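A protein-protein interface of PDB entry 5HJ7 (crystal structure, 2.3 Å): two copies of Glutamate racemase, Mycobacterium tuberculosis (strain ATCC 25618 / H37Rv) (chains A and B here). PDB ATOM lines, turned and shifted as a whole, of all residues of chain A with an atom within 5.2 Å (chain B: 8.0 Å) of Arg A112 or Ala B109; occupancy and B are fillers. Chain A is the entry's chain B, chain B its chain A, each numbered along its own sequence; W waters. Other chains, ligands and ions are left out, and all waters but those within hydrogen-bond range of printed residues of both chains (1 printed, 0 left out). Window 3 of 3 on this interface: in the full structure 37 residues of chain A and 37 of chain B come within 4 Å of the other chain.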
ATOM      1  N   ALA A 110      20.017  16.380  31.047  1.00  0.00           N
ATOM      2  CA  ALA A 110      19.465  17.665  30.643  1.00  0.00           C
ATOM      3  C   ALA A 110      19.073  17.730  29.172  1.00  0.00           C
ATOM      4  O   ALA A 110      18.307  18.625  28.795  1.00  0.00           O
ATOM      5  CB  ALA A 110      20.464  18.787  30.944  1.00  0.00           C
ATOM      6  N   THR A 111      19.567  16.826  28.332  1.00  0.00           N
ATOM      7  CA  THR A 111      19.271  16.916  26.909  1.00  0.00           C
ATOM      8  C   THR A 111      17.812  16.545  26.628  1.00  0.00           C
ATOM      9  O   THR A 111      17.208  15.706  27.309  1.00  0.00           O
ATOM     10  CB  THR A 111      20.222  16.021  26.110  1.00  0.00           C
ATOM     11  OG1 THR A 111      20.001  16.202  24.702  1.00  0.00           O
ATOM     12  CG2 THR A 111      20.041  14.555  26.487  1.00  0.00           C
ATOM     13  N   ARG A 112      17.230  17.216  25.635  1.00  0.00           N
ATOM     14  CA  ARG A 112      15.888  16.868  25.174  1.00  0.00           C
ATOM     15  C   ARG A 112      15.900  16.044  23.886  1.00  0.00           C
ATOM     16  O   ARG A 112      15.102  15.115  23.747  1.00  0.00           O
ATOM     17  CB  ARG A 112      15.037  18.133  24.970  1.00  0.00           C
ATOM     18  CG  ARG A 112      14.601  18.853  26.267  1.00  0.00           C
ATOM     19  CD  ARG A 112      15.239  20.236  26.385  1.00  0.00           C
ATOM     20  NE  ARG A 112      16.619  20.110  26.794  1.00  0.00           N
ATOM     21  CZ  ARG A 112      17.641  20.813  26.303  1.00  0.00           C
ATOM     22  NH1 ARG A 112      17.463  21.730  25.356  1.00  0.00           N
ATOM     23  NH2 ARG A 112      18.859  20.585  26.774  1.00  0.00           N
ATOM     24  N   ASN A 113      16.794  16.338  22.946  1.00  0.00           N
ATOM     25  CA  ASN A 113      16.797  15.658  21.659  1.00  0.00           C
ATOM     26  C   ASN A 113      17.898  14.611  21.552  1.00  0.00           C
ATOM     27  O   ASN A 113      18.098  14.046  20.475  1.00  0.00           O
ATOM     28  CB  ASN A 113      16.907  16.676  20.516  1.00  0.00           C
ATOM     29  CG  ASN A 113      18.251  17.408  20.476  1.00  0.00           C
ATOM     30  OD1 ASN A 113      19.189  17.090  21.213  1.00  0.00           O
ATOM     31  ND2 ASN A 113      18.344  18.394  19.593  1.00  0.00           N
ATOM     32  N   GLY A 114      18.615  14.343  22.642  1.00  0.00           N
ATOM     33  CA  GLY A 114      19.663  13.352  22.629  1.00  0.00           C
ATOM     34  C   GLY A 114      20.937  13.761  21.932  1.00  0.00           C
ATOM     35  O   GLY A 114      21.808  12.910  21.742  1.00  0.00           O
ATOM     36  N   ASP A 181      21.567  20.248  21.615  1.00  0.00           N
ATOM     37  CA  ASP A 181      20.836  21.120  22.519  1.00  0.00           C
ATOM     38  C   ASP A 181      21.481  21.194  23.894  1.00  0.00           C
ATOM     39  O   ASP A 181      20.928  21.841  24.794  1.00  0.00           O
ATOM     40  CB  ASP A 181      19.371  20.669  22.635  1.00  0.00           C
ATOM     41  CG  ASP A 181      19.212  19.280  23.242  1.00  0.00           C
ATOM     42  OD1 ASP A 181      20.179  18.714  23.805  1.00  0.00           O
ATOM     43  OD2 ASP A 181      18.077  18.760  23.182  1.00  0.00           O
ATOM     44  N   THR A 182      22.631  20.539  24.074  1.00  0.00           N
ATOM     45  CA  THR A 182      23.367  20.511  25.325  1.00  0.00           C
ATOM     46  C   THR A 182      24.855  20.574  25.009  1.00  0.00           C
ATOM     47  O   THR A 182      25.346  19.845  24.144  1.00  0.00           O
ATOM     48  CB  THR A 182      23.050  19.245  26.135  1.00  0.00           C
ATOM     49  OG1 THR A 182      21.636  19.155  26.352  1.00  0.00           O
ATOM     50  CG2 THR A 182      23.738  19.288  27.492  1.00  0.00           C
ATOM     51  N   GLU A 203      19.546  30.195  22.218  1.00  0.00           N
ATOM     52  CA  GLU A 203      18.927  30.061  23.531  1.00  0.00           C
ATOM     53  C   GLU A 203      18.439  28.649  23.855  1.00  0.00           C
ATOM     54  O   GLU A 203      18.193  28.362  25.030  1.00  0.00           O
ATOM     55  CB  GLU A 203      17.758  31.032  23.658  1.00  0.00           C
ATOM     56  CG  GLU A 203      18.060  32.209  24.584  1.00  0.00           C
ATOM     57  CD  GLU A 203      16.785  32.878  25.101  1.00  0.00           C
ATOM     58  OE1 GLU A 203      15.681  32.550  24.596  1.00  0.00           O
ATOM     59  OE2 GLU A 203      16.890  33.728  26.017  1.00  0.00           O
ATOM     60  N   ASN A 204      18.282  27.761  22.870  1.00  0.00           N
ATOM     61  CA  ASN A 204      17.837  26.408  23.189  1.00  0.00           C
ATOM     62  C   ASN A 204      18.973  25.490  23.641  1.00  0.00           C
ATOM     63  O   ASN A 204      18.712  24.337  23.990  1.00  0.00           O
ATOM     64  CB  ASN A 204      17.111  25.760  21.994  1.00  0.00           C
ATOM     65  CG  ASN A 204      16.312  24.496  22.397  1.00  0.00           C
ATOM     66  OD1 ASN A 204      16.557  23.386  21.899  1.00  0.00           O
ATOM     67  ND2 ASN A 204      15.378  24.665  23.330  1.00  0.00           N
ATOM     68  N   THR A 206      21.523  24.154  26.264  1.00  0.00           N
ATOM     69  CA  THR A 206      21.853  24.152  27.693  1.00  0.00           C
ATOM     70  C   THR A 206      23.357  23.968  27.865  1.00  0.00           C
ATOM     71  O   THR A 206      23.908  22.935  27.460  1.00  0.00           O
ATOM     72  CB  THR A 206      21.132  23.028  28.442  1.00  0.00           C
ATOM     73  OG1 THR A 206      19.713  23.140  28.275  1.00  0.00           O
ATOM     74  CG2 THR A 206      21.482  23.067  29.943  1.00  0.00           C
ATOM     75  N   PRO B 102      15.325  36.196  32.379  1.00  0.00           N
ATOM     76  CA  PRO B 102      16.336  35.289  31.799  1.00  0.00           C
ATOM     77  C   PRO B 102      16.232  33.869  32.331  1.00  0.00           C
ATOM     78  O   PRO B 102      16.389  32.912  31.563  1.00  0.00           O
ATOM     79  CB  PRO B 102      17.667  35.961  32.173  1.00  0.00           C
ATOM     80  CG  PRO B 102      17.312  37.432  32.251  1.00  0.00           C
ATOM     81  CD  PRO B 102      15.945  37.439  32.880  1.00  0.00           C
ATOM     82  N   ALA B 103      15.938  33.704  33.619  1.00  0.00           N
ATOM     83  CA  ALA B 103      15.759  32.365  34.172  1.00  0.00           C
ATOM     84  C   ALA B 103      14.493  31.717  33.640  1.00  0.00           C
ATOM     85  O   ALA B 103      14.483  30.515  33.362  1.00  0.00           O
ATOM     86  CB  ALA B 103      15.722  32.411  35.701  1.00  0.00           C
ATOM     87  N   VAL B 104      13.407  32.494  33.517  1.00  0.00           N
ATOM     88  CA  VAL B 104      12.154  31.950  32.986  1.00  0.00           C
ATOM     89  C   VAL B 104      12.389  31.364  31.600  1.00  0.00           C
ATOM     90  O   VAL B 104      11.991  30.230  31.308  1.00  0.00           O
ATOM     91  CB  VAL B 104      11.048  33.028  32.968  1.00  0.00           C
ATOM     92  CG1 VAL B 104       9.884  32.619  32.035  1.00  0.00           C
ATOM     93  CG2 VAL B 104      10.512  33.302  34.383  1.00  0.00           C
ATOM     94  N   ARG B 105      13.063  32.128  30.734  1.00  0.00           N
ATOM     95  CA  ARG B 105      13.347  31.664  29.380  1.00  0.00           C
ATOM     96  C   ARG B 105      14.242  30.424  29.381  1.00  0.00           C
ATOM     97  O   ARG B 105      14.021  29.496  28.591  1.00  0.00           O
ATOM     98  CB  ARG B 105      13.979  32.793  28.561  1.00  0.00           C
ATOM     99  CG  ARG B 105      12.968  33.845  28.077  1.00  0.00           C
ATOM    100  CD  ARG B 105      13.595  34.819  27.083  1.00  0.00           C
ATOM    101  NE  ARG B 105      14.623  35.636  27.723  1.00  0.00           N
ATOM    102  CZ  ARG B 105      14.400  36.849  28.228  1.00  0.00           C
ATOM    103  NH1 ARG B 105      13.180  37.385  28.148  1.00  0.00           N
ATOM    104  NH2 ARG B 105      15.393  37.532  28.803  1.00  0.00           N
ATOM    105  N   ARG B 106      15.258  30.386  30.255  1.00  0.00           N
ATOM    106  CA  ARG B 106      16.110  29.197  30.335  1.00  0.00           C
ATOM    107  C   ARG B 106      15.320  27.977  30.799  1.00  0.00           C
ATOM    108  O   ARG B 106      15.464  26.880  30.235  1.00  0.00           O
ATOM    109  CB  ARG B 106      17.296  29.441  31.273  1.00  0.00           C
ATOM    110  CG  ARG B 106      18.333  28.270  31.305  1.00  0.00           C
ATOM    111  CD  ARG B 106      19.036  28.108  29.943  1.00  0.00           C
ATOM    112  NE  ARG B 106      19.456  29.418  29.465  1.00  0.00           N
ATOM    113  CZ  ARG B 106      19.715  29.720  28.198  1.00  0.00           C
ATOM    114  NH1 ARG B 106      19.613  28.786  27.261  1.00  0.00           N
ATOM    115  NH2 ARG B 106      20.082  30.956  27.870  1.00  0.00           N
ATOM    116  N   ALA B 107      14.480  28.154  31.831  1.00  0.00           N
ATOM    117  CA  ALA B 107      13.716  27.039  32.399  1.00  0.00           C
ATOM    118  C   ALA B 107      12.747  26.436  31.380  1.00  0.00           C
ATOM    119  O   ALA B 107      12.583  25.211  31.313  1.00  0.00           O
ATOM    120  CB  ALA B 107      12.963  27.507  33.649  1.00  0.00           C
ATOM    121  N   VAL B 108      12.092  27.276  30.579  1.00  0.00           N
ATOM    122  CA  VAL B 108      11.198  26.762  29.543  1.00  0.00           C
ATOM    123  C   VAL B 108      11.982  26.014  28.464  1.00  0.00           C
ATOM    124  O   VAL B 108      11.496  25.019  27.911  1.00  0.00           O
ATOM    125  CB  VAL B 108      10.356  27.918  28.956  1.00  0.00           C
ATOM    126  CG1 VAL B 108       9.633  27.488  27.690  1.00  0.00           C
ATOM    127  CG2 VAL B 108       9.353  28.412  29.992  1.00  0.00           C
ATOM    128  N   ALA B 109      13.202  26.457  28.158  1.00  0.00           N
ATOM    129  CA  ALA B 109      14.024  25.748  27.182  1.00  0.00           C
ATOM    130  C   ALA B 109      14.639  24.477  27.749  1.00  0.00           C
ATOM    131  O   ALA B 109      14.959  23.557  26.985  1.00  0.00           O
ATOM    132  CB  ALA B 109      15.146  26.654  26.673  1.00  0.00           C
ATOM    133  N   ALA B 110      14.843  24.410  29.063  1.00  0.00           N
ATOM    134  CA  ALA B 110      15.606  23.320  29.655  1.00  0.00           C
ATOM    135  C   ALA B 110      14.749  22.158  30.129  1.00  0.00           C
ATOM    136  O   ALA B 110      15.293  21.076  30.380  1.00  0.00           O
ATOM    137  CB  ALA B 110      16.431  23.837  30.832  1.00  0.00           C
ATOM    138  N   THR B 111      13.438  22.342  30.275  1.00  0.00           N
ATOM    139  CA  THR B 111      12.610  21.292  30.857  1.00  0.00           C
ATOM    140  C   THR B 111      12.326  20.192  29.839  1.00  0.00           C
ATOM    141  O   THR B 111      12.272  20.432  28.628  1.00  0.00           O
ATOM    142  CB  THR B 111      11.300  21.865  31.409  1.00  0.00           C
ATOM    143  OG1 THR B 111      10.595  20.845  32.127  1.00  0.00           O
ATOM    144  CG2 THR B 111      10.413  22.420  30.296  1.00  0.00           C
ATOM    145  N   ARG B 112      12.193  18.963  30.348  1.00  0.00           N
ATOM    146  CA  ARG B 112      11.917  17.773  29.548  1.00  0.00           C
ATOM    147  C   ARG B 112      10.484  17.287  29.670  1.00  0.00           C
ATOM    148  O   ARG B 112       9.925  16.797  28.694  1.00  0.00           O
ATOM    149  CB  ARG B 112      12.863  16.624  29.935  1.00  0.00           C
ATOM    150  CG  ARG B 112      14.305  16.843  29.499  1.00  0.00           C
ATOM    151  CD  ARG B 112      15.252  16.818  30.681  1.00  0.00           C
ATOM    152  NE  ARG B 112      15.098  17.968  31.551  1.00  0.00           N
ATOM    153  CZ  ARG B 112      15.210  17.932  32.874  1.00  0.00           C
ATOM    154  NH1 ARG B 112      15.062  19.047  33.559  1.00  0.00           N
ATOM    155  NH2 ARG B 112      15.455  16.797  33.512  1.00  0.00           N
ATOM    156  N   ASN B 113       9.871  17.392  30.848  1.00  0.00           N
ATOM    157  CA  ASN B 113       8.505  16.936  31.028  1.00  0.00           C
ATOM    158  C   ASN B 113       7.531  18.088  31.222  1.00  0.00           C
ATOM    159  O   ASN B 113       6.334  17.844  31.414  1.00  0.00           O
ATOM    160  CB  ASN B 113       8.416  15.954  32.207  1.00  0.00           C
ATOM    161  CG  ASN B 113       8.709  16.603  33.545  1.00  0.00           C
ATOM    162  OD1 ASN B 113       8.998  17.804  33.633  1.00  0.00           O
ATOM    163  ND2 ASN B 113       8.630  15.808  34.607  1.00  0.00           N
ATOM    164  N   ILE B 116       7.853  22.580  36.056  1.00  0.00           N
ATOM    165  CA  ILE B 116       8.845  23.560  36.476  1.00  0.00           C
ATOM    166  C   ILE B 116       8.491  24.053  37.873  1.00  0.00           C
ATOM    167  O   ILE B 116       7.329  24.358  38.167  1.00  0.00           O
ATOM    168  CB  ILE B 116       8.916  24.749  35.492  1.00  0.00           C
ATOM    169  CG1 ILE B 116       9.187  24.278  34.072  1.00  0.00           C
ATOM    170  CG2 ILE B 116       9.974  25.774  35.921  1.00  0.00           C
ATOM    171  CD1 ILE B 116       9.142  25.421  33.080  1.00  0.00           C
ATOM    172  N   PHE B 134       5.292  32.541  33.576  1.00  0.00           N
ATOM    173  CA  PHE B 134       5.256  31.229  32.960  1.00  0.00           C
ATOM    174  C   PHE B 134       3.933  30.915  32.272  1.00  0.00           C
ATOM    175  O   PHE B 134       3.858  29.893  31.578  1.00  0.00           O
ATOM    176  CB  PHE B 134       5.524  30.156  34.003  1.00  0.00           C
ATOM    177  CG  PHE B 134       6.973  29.876  34.231  1.00  0.00           C
ATOM    178  CD1 PHE B 134       7.740  29.294  33.240  1.00  0.00           C
ATOM    179  CD2 PHE B 134       7.563  30.154  35.463  1.00  0.00           C
ATOM    180  CE1 PHE B 134       9.080  29.015  33.459  1.00  0.00           C
ATOM    181  CE2 PHE B 134       8.894  29.887  35.685  1.00  0.00           C
ATOM    182  CZ  PHE B 134       9.657  29.313  34.684  1.00  0.00           C
ATOM    183  N   ALA B 137       3.751  29.772  28.643  1.00  0.00           N
ATOM    184  CA  ALA B 137       4.481  28.579  28.236  1.00  0.00           C
ATOM    185  C   ALA B 137       3.492  27.441  28.019  1.00  0.00           C
ATOM    186  O   ALA B 137       2.789  27.041  28.954  1.00  0.00           O
ATOM    187  CB  ALA B 137       5.531  28.204  29.282  1.00  0.00           C
ATOM    188  N   THR B 140       3.208  23.505  30.232  1.00  0.00           N
ATOM    189  CA  THR B 140       3.997  23.564  31.449  1.00  0.00           C
ATOM    190  C   THR B 140       3.083  23.725  32.648  1.00  0.00           C
ATOM    191  O   THR B 140       2.017  24.341  32.563  1.00  0.00           O
ATOM    192  CB  THR B 140       5.036  24.711  31.455  1.00  0.00           C
ATOM    193  OG1 THR B 140       4.375  25.979  31.523  1.00  0.00           O
ATOM    194  CG2 THR B 140       5.932  24.658  30.218  1.00  0.00           C
ATOM    195  N   ASP B 181      11.077  18.675  36.926  1.00  0.00           N
ATOM    196  CA  ASP B 181      12.401  18.326  36.434  1.00  0.00           C
ATOM    197  C   ASP B 181      13.281  19.554  36.241  1.00  0.00           C
ATOM    198  O   ASP B 181      14.427  19.422  35.794  1.00  0.00           O
ATOM    199  CB  ASP B 181      12.302  17.494  35.137  1.00  0.00           C
ATOM    200  CG  ASP B 181      11.955  18.321  33.881  1.00  0.00           C
ATOM    201  OD1 ASP B 181      11.680  19.534  33.960  1.00  0.00           O
ATOM    202  OD2 ASP B 181      11.954  17.722  32.784  1.00  0.00           O
ATOM    203  N   THR B 182      12.780  20.740  36.603  1.00  0.00           N
ATOM    204  CA  THR B 182      13.489  22.001  36.437  1.00  0.00           C
ATOM    205  C   THR B 182      13.103  22.908  37.591  1.00  0.00           C
ATOM    206  O   THR B 182      11.924  23.002  37.935  1.00  0.00           O
ATOM    207  CB  THR B 182      13.154  22.675  35.095  1.00  0.00           C
ATOM    208  OG1 THR B 182      13.401  21.756  34.027  1.00  0.00           O
ATOM    209  CG2 THR B 182      14.023  23.890  34.884  1.00  0.00           C
ATOM    210  N   THR B 206      17.041  19.916  36.843  1.00  0.00           N
ATOM    211  CA  THR B 206      17.946  20.965  36.375  1.00  0.00           C
ATOM    212  C   THR B 206      17.711  22.243  37.167  1.00  0.00           C
ATOM    213  O   THR B 206      16.627  22.835  37.086  1.00  0.00           O
ATOM    214  CB  THR B 206      17.744  21.249  34.888  1.00  0.00           C
ATOM    215  OG1 THR B 206      17.993  20.063  34.124  1.00  0.00           O
ATOM    216  CG2 THR B 206      18.695  22.353  34.426  1.00  0.00           C
HETATM  217  O   HOH W   1      16.798  29.988  26.536  1.00  0.00           O
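Among the printed residues, pairs that only touch across the chains: Arg A112 with Ala B109 (3.4 Å), Arg A112 with Thr B111 (3.7 Å), Thr A111 with Arg B112 (3.8 Å), Arg A112 with Arg B112 (3.8 Å), Asn A204 with Ala B109 (3.8 Å), Glu A203 with Ala B109 (3.9 Å) and Arg A112 with Ala B110 (3.9 Å).
Water W1 lies within hydrogen-bond range of the backbone carbonyl oxygen (O) of Glu A203 (2.6 Å), the guanidinium group (NH1) of Arg B106 (3.1 Å) and the backbone carbonyl oxygen (O) of Arg B105 (3.5 Å).
The guanidinium group (NE) of Arg B105 lies within salt-bridge range of the side-chain carboxylate (OE2) of Glu A203, at 3.4 Å.
The guanidinium group (NH1) of Arg B106 sits at hydrogen-bond distance from the backbone carbonyl oxygen (O) of Glu A203, 2.7 Å away.
Of chain B, only Ala B109, Ala B110, Thr B111 and Arg B112 come within 4 Å of Arg A112.
Pro B102 touches none of the printed residues of chain A.
Of the printed residues of chain A, Arg B105 touches Glu A203 (3.4 Å).
Printed residues of chain A within 4 Å of Arg B106: Glu A203 (2.7 Å).
Val B108 touches none of the printed residues of chain A.
Ala B109 touches just these residues of chain A: Arg A112, Glu A203 and Asn A204.
Printed residues of chain A within 4 Å of Arg B112: Thr A111 and Arg A112.
The nearest residue of chain B that does not touch Arg A112 is Val B108 (6.3 Å).
The nearest residue of chain A that does not touch Ala B109 is Thr A206 (4.9 Å).
Thr A111 touches Arg B112, and with the chains exchanged Arg A112 touches Thr B111.
Arg A112 touches Ala B110, but with the chains exchanged Ala A110 does not touch Arg B112 (4.02 Å).
Arg A112 touches its own counterpart, Arg B112.
Of the 9 pairs that touch across the chains among the printed residues, 3 have their exchanged pair printed and touching as well.
Of the 19 printed residues of chain B, 6 touch a printed residue of chain A.
Printed residues of chain B that touch a printed residue of chain A: Arg B105, Arg B106, Ala B109, Ala B110, Thr B111 and Arg B112.
Hydrophobic or aromatic side chains of chain B within 4 Å of the printed part of chain A: Ala B109.
Among the printed residues, 9 pairs touch across the chains.
Among the printed residues, Asp or Glu carboxylates within 4 Å of a Lys or Arg side-chain nitrogen of the other chain: Glu A203 with Arg B105.
The backbone carbonyl oxygen (O) of Ala B110 lies within hydrogen-bond range of the guanidinium group (NE) of Arg B112, at 3.3 Å.
OD2 of Asp B181 is in salt-bridge range of NE of Arg B112, 3.4 Å away.
The guanidinium group of Arg B112 sits at hydrogen-bond distance from the side-chain hydroxyl of Thr B182, 3.2 Å away.
The guanidinium group (NH2) of Arg A112 sits at hydrogen-bond distance from the backbone carbonyl oxygen (O) of Ala A110 (2.9 Å).
The side-chain hydroxyl (OG1) of Thr A111 is in hydrogen-bond range of the backbone NH (N) of Gly A114 (3.1 Å).
The side-chain carboxylate of Asp A181 lies within salt-bridge range of the guanidinium group of Arg A112 (3.7 Å).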
